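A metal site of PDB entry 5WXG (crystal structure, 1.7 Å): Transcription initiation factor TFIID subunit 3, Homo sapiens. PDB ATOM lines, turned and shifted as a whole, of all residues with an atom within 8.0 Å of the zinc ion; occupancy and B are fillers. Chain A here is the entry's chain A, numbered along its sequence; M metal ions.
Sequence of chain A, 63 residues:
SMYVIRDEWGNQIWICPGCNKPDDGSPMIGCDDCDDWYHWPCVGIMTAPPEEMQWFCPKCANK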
ATOM      1  N   PRO A  17     -11.885  20.503  18.855  1.00  0.00           N
ATOM      2  CA  PRO A  17     -12.959  21.290  19.484  1.00  0.00           C
ATOM      3  C   PRO A  17     -13.518  22.361  18.580  1.00  0.00           C
ATOM      4  O   PRO A  17     -14.609  22.872  18.867  1.00  0.00           O
ATOM      5  CB  PRO A  17     -12.286  21.883  20.723  1.00  0.00           C
ATOM      6  CG  PRO A  17     -11.020  21.010  20.932  1.00  0.00           C
ATOM      7  CD  PRO A  17     -10.594  20.677  19.542  1.00  0.00           C
ATOM      8  N   GLY A  30      -1.476  21.454  18.468  1.00  0.00           N
ATOM      9  CA  GLY A  30      -1.832  21.192  19.854  1.00  0.00           C
ATOM     10  C   GLY A  30      -1.645  22.414  20.730  1.00  0.00           C
ATOM     11  O   GLY A  30      -0.622  23.103  20.630  1.00  0.00           O
ATOM     12  N   CYS A  31      -2.614  22.666  21.605  1.00  0.00           N
ATOM     13  CA  CYS A  31      -2.528  23.826  22.488  1.00  0.00           C
ATOM     14  C   CYS A  31      -1.411  23.649  23.503  1.00  0.00           C
ATOM     15  O   CYS A  31      -1.299  22.599  24.146  1.00  0.00           O
ATOM     16  CB  CYS A  31      -3.854  24.022  23.212  1.00  0.00           C
ATOM     17  SG  CYS A  31      -3.805  25.486  24.257  1.00  0.00           S
ATOM     18  N   ASP A  32      -0.581  24.671  23.653  1.00  0.00           N
ATOM     19  CA  ASP A  32       0.537  24.607  24.583  1.00  0.00           C
ATOM     20  C   ASP A  32       0.141  24.826  26.036  1.00  0.00           C
ATOM     21  O   ASP A  32       1.004  24.758  26.915  1.00  0.00           O
ATOM     22  CB  ASP A  32       1.625  25.619  24.178  1.00  0.00           C
ATOM     23  CG  ASP A  32       2.417  25.151  22.979  1.00  0.00           C
ATOM     24  OD1 ASP A  32       2.473  23.927  22.741  1.00  0.00           O
ATOM     25  OD2 ASP A  32       3.005  26.005  22.279  1.00  0.00           O
ATOM     26  N   ASP A  33      -1.143  25.067  26.326  1.00  0.00           N
ATOM     27  CA  ASP A  33      -1.645  25.088  27.687  1.00  0.00           C
ATOM     28  C   ASP A  33      -2.472  23.834  27.956  1.00  0.00           C
ATOM     29  O   ASP A  33      -2.042  22.965  28.713  1.00  0.00           O
ATOM     30  CB  ASP A  33      -2.452  26.377  27.951  1.00  0.00           C
ATOM     31  CG  ASP A  33      -2.912  26.519  29.406  1.00  0.00           C
ATOM     32  OD1 ASP A  33      -3.011  25.515  30.136  1.00  0.00           O
ATOM     33  OD2 ASP A  33      -3.200  27.666  29.820  1.00  0.00           O
ATOM     34  N   CYS A  34      -3.639  23.688  27.316  1.00  0.00           N
ATOM     35  CA  CYS A  34      -4.567  22.608  27.649  1.00  0.00           C
ATOM     36  C   CYS A  34      -4.345  21.316  26.849  1.00  0.00           C
ATOM     37  O   CYS A  34      -4.920  20.289  27.208  1.00  0.00           O
ATOM     38  CB  CYS A  34      -6.022  23.068  27.437  1.00  0.00           C
ATOM     39  SG  CYS A  34      -6.527  23.249  25.718  1.00  0.00           S
ATOM     40  N   ASP A  35      -3.551  21.355  25.769  1.00  0.00           N
ATOM     41  CA  ASP A  35      -3.215  20.177  24.953  1.00  0.00           C
ATOM     42  C   ASP A  35      -4.418  19.542  24.240  1.00  0.00           C
ATOM     43  O   ASP A  35      -4.379  18.354  23.895  1.00  0.00           O
ATOM     44  CB  ASP A  35      -2.464  19.114  25.783  1.00  0.00           C
ATOM     45  CG  ASP A  35      -1.592  18.195  24.932  1.00  0.00           C
ATOM     46  OD1 ASP A  35      -0.937  18.670  23.966  1.00  0.00           O
ATOM     47  OD2 ASP A  35      -1.545  16.980  25.229  1.00  0.00           O
ATOM     48  N   ASP A  36      -5.496  20.308  24.008  1.00  0.00           N
ATOM     49  CA  ASP A  36      -6.461  19.952  22.969  1.00  0.00           C
ATOM     50  C   ASP A  36      -5.785  20.076  21.608  1.00  0.00           C
ATOM     51  O   ASP A  36      -4.883  20.895  21.425  1.00  0.00           O
ATOM     52  CB  ASP A  36      -7.686  20.880  23.007  1.00  0.00           C
ATOM     53  CG  ASP A  36      -8.627  20.572  24.161  1.00  0.00           C
ATOM     54  OD1 ASP A  36      -8.502  19.497  24.787  1.00  0.00           O
ATOM     55  OD2 ASP A  36      -9.521  21.408  24.416  1.00  0.00           O
ATOM     56  N   TRP A  37      -6.235  19.279  20.644  1.00  0.00           N
ATOM     57  CA  TRP A  37      -5.672  19.290  19.298  1.00  0.00           C
ATOM     58  C   TRP A  37      -6.739  19.682  18.280  1.00  0.00           C
ATOM     59  O   TRP A  37      -7.873  19.222  18.347  1.00  0.00           O
ATOM     60  CB  TRP A  37      -5.046  17.924  18.948  1.00  0.00           C
ATOM     61  CG  TRP A  37      -3.716  17.751  19.626  1.00  0.00           C
ATOM     62  CD1 TRP A  37      -3.492  17.471  20.942  1.00  0.00           C
ATOM     63  CD2 TRP A  37      -2.427  17.901  19.016  1.00  0.00           C
ATOM     64  NE1 TRP A  37      -2.137  17.419  21.190  1.00  0.00           N
ATOM     65  CE2 TRP A  37      -1.462  17.674  20.024  1.00  0.00           C
ATOM     66  CE3 TRP A  37      -1.993  18.193  17.724  1.00  0.00           C
ATOM     67  CZ2 TRP A  37      -0.089  17.751  19.781  1.00  0.00           C
ATOM     68  CZ3 TRP A  37      -0.619  18.257  17.479  1.00  0.00           C
ATOM     69  CH2 TRP A  37       0.305  18.037  18.501  1.00  0.00           C
ATOM     70  N   TYR A  38      -6.350  20.523  17.328  1.00  0.00           N
ATOM     71  CA  TYR A  38      -7.248  21.134  16.350  1.00  0.00           C
ATOM     72  C   TYR A  38      -6.761  20.862  14.925  1.00  0.00           C
ATOM     73  O   TYR A  38      -5.554  20.887  14.679  1.00  0.00           O
ATOM     74  CB  TYR A  38      -7.319  22.664  16.541  1.00  0.00           C
ATOM     75  CG  TYR A  38      -8.105  23.177  17.732  1.00  0.00           C
ATOM     76  CD1 TYR A  38      -7.622  23.040  19.030  1.00  0.00           C
ATOM     77  CD2 TYR A  38      -9.324  23.829  17.547  1.00  0.00           C
ATOM     78  CE1 TYR A  38      -8.346  23.530  20.123  1.00  0.00           C
ATOM     79  CE2 TYR A  38     -10.042  24.337  18.620  1.00  0.00           C
ATOM     80  CZ  TYR A  38      -9.554  24.181  19.902  1.00  0.00           C
ATOM     81  OH  TYR A  38     -10.290  24.665  20.978  1.00  0.00           O
ATOM     82  N   TRP A  55       1.781  28.176  20.552  1.00  0.00           N
ATOM     83  CA  TRP A  55       0.423  28.270  20.056  1.00  0.00           C
ATOM     84  C   TRP A  55      -0.561  27.899  21.165  1.00  0.00           C
ATOM     85  O   TRP A  55      -0.363  26.911  21.892  1.00  0.00           O
ATOM     86  CB  TRP A  55       0.197  27.381  18.836  1.00  0.00           C
ATOM     87  CG  TRP A  55      -1.180  27.561  18.228  1.00  0.00           C
ATOM     88  CD1 TRP A  55      -1.537  28.517  17.317  1.00  0.00           C
ATOM     89  CD2 TRP A  55      -2.363  26.789  18.490  1.00  0.00           C
ATOM     90  NE1 TRP A  55      -2.854  28.376  16.983  1.00  0.00           N
ATOM     91  CE2 TRP A  55      -3.395  27.338  17.699  1.00  0.00           C
ATOM     92  CE3 TRP A  55      -2.651  25.702  19.318  1.00  0.00           C
ATOM     93  CZ2 TRP A  55      -4.684  26.835  17.709  1.00  0.00           C
ATOM     94  CZ3 TRP A  55      -3.935  25.181  19.312  1.00  0.00           C
ATOM     95  CH2 TRP A  55      -4.949  25.753  18.518  1.00  0.00           C
ATOM     96  N   PHE A  56      -1.627  28.681  21.281  1.00  0.00           N
ATOM     97  CA  PHE A  56      -2.694  28.416  22.249  1.00  0.00           C
ATOM     98  C   PHE A  56      -4.041  28.420  21.538  1.00  0.00           C
ATOM     99  O   PHE A  56      -4.257  29.174  20.579  1.00  0.00           O
ATOM    100  CB  PHE A  56      -2.686  29.445  23.389  1.00  0.00           C
ATOM    101  CG  PHE A  56      -1.382  29.490  24.131  1.00  0.00           C
ATOM    102  CD1 PHE A  56      -1.146  28.636  25.199  1.00  0.00           C
ATOM    103  CD2 PHE A  56      -0.387  30.375  23.753  1.00  0.00           C
ATOM    104  CE1 PHE A  56       0.061  28.668  25.867  1.00  0.00           C
ATOM    105  CE2 PHE A  56       0.814  30.413  24.424  1.00  0.00           C
ATOM    106  CZ  PHE A  56       1.038  29.566  25.486  1.00  0.00           C
ATOM    107  N   CYS A  57      -4.944  27.567  22.004  1.00  0.00           N
ATOM    108  CA  CYS A  57      -6.264  27.429  21.406  1.00  0.00           C
ATOM    109  C   CYS A  57      -7.123  28.633  21.774  1.00  0.00           C
ATOM    110  O   CYS A  57      -6.744  29.430  22.635  1.00  0.00           O
ATOM    111  CB  CYS A  57      -6.917  26.125  21.887  1.00  0.00           C
ATOM    112  SG  CYS A  57      -7.514  26.190  23.581  1.00  0.00           S
ATOM    113  N   PRO A  58      -8.278  28.791  21.121  1.00  0.00           N
ATOM    114  CA  PRO A  58      -9.078  30.000  21.395  1.00  0.00           C
ATOM    115  C   PRO A  58      -9.547  30.108  22.828  1.00  0.00           C
ATOM    116  O   PRO A  58      -9.741  31.233  23.314  1.00  0.00           O
ATOM    117  CB  PRO A  58     -10.247  29.868  20.407  1.00  0.00           C
ATOM    118  CG  PRO A  58      -9.643  29.071  19.267  1.00  0.00           C
ATOM    119  CD  PRO A  58      -8.821  28.039  19.980  1.00  0.00           C
ATOM    120  N   LYS A  59      -9.770  28.977  23.512  1.00  0.00           N
ATOM    121  CA  LYS A  59     -10.188  29.052  24.903  1.00  0.00           C
ATOM    122  C   LYS A  59      -9.056  29.526  25.793  1.00  0.00           C
ATOM    123  O   LYS A  59      -9.269  30.336  26.707  1.00  0.00           O
ATOM    124  CB  LYS A  59     -10.688  27.685  25.390  1.00  0.00           C
ATOM    125  CG  LYS A  59     -11.682  27.001  24.462  1.00  0.00           C
ATOM    126  CD  LYS A  59     -12.142  25.670  25.067  1.00  0.00           C
ATOM    127  CE  LYS A  59     -12.684  24.704  24.019  1.00  0.00           C
ATOM    128  NZ  LYS A  59     -13.990  25.124  23.435  1.00  0.00           N
ATOM    129  N   CYS A  60      -7.852  29.016  25.575  1.00  0.00           N
ATOM    130  CA  CYS A  60      -6.694  29.429  26.353  1.00  0.00           C
ATOM    131  C   CYS A  60      -6.188  30.809  25.983  1.00  0.00           C
ATOM    132  O   CYS A  60      -5.512  31.450  26.790  1.00  0.00           O
ATOM    133  CB  CYS A  60      -5.570  28.398  26.211  1.00  0.00           C
ATOM    134  SG  CYS A  60      -5.996  26.829  27.001  1.00  0.00           S
ATOM    135  N   ALA A  61      -6.512  31.294  24.777  1.00  0.00           N
ATOM    136  CA  ALA A  61      -6.109  32.633  24.373  1.00  0.00           C
ATOM    137  C   ALA A  61      -7.042  33.718  24.923  1.00  0.00           C
ATOM    138  O   ALA A  61      -6.735  34.903  24.779  1.00  0.00           O
ATOM    139  CB  ALA A  61      -6.060  32.740  22.851  1.00  0.00           C
HETATM  140 ZN    ZN M   1      -5.999  25.374  25.124  1.00  0.00          ZN
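N of Asp 36 sits close to SG of Cys 34, at 3.6 Å.
SG of Cys 57 lies close to N of Lys 59 (3.6 Å).
SG of Cys 31 sits close to N of Asp 33, 3.4 Å away.
N of Cys 31 is in hydrogen-bond range of O of Asp 36 (2.9 Å).
Within 4 Å of the zinc ion: Cys 31, Cys 34, Cys 57 and Cys 60.
Along chain A the residues within 4 Å of the zinc ion span positions 31 to 60.
The nearest printed residue that does not touch the zinc ion is Asp 33 (4.6 Å).
The zinc ion is bound by the side-chain sulfur of Cys 34, the side-chain sulfur of Cys 57, the side-chain sulfur of Cys 31 and the side-chain sulfur of Cys 60.
The zinc ion has four donor atoms within binding distance.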
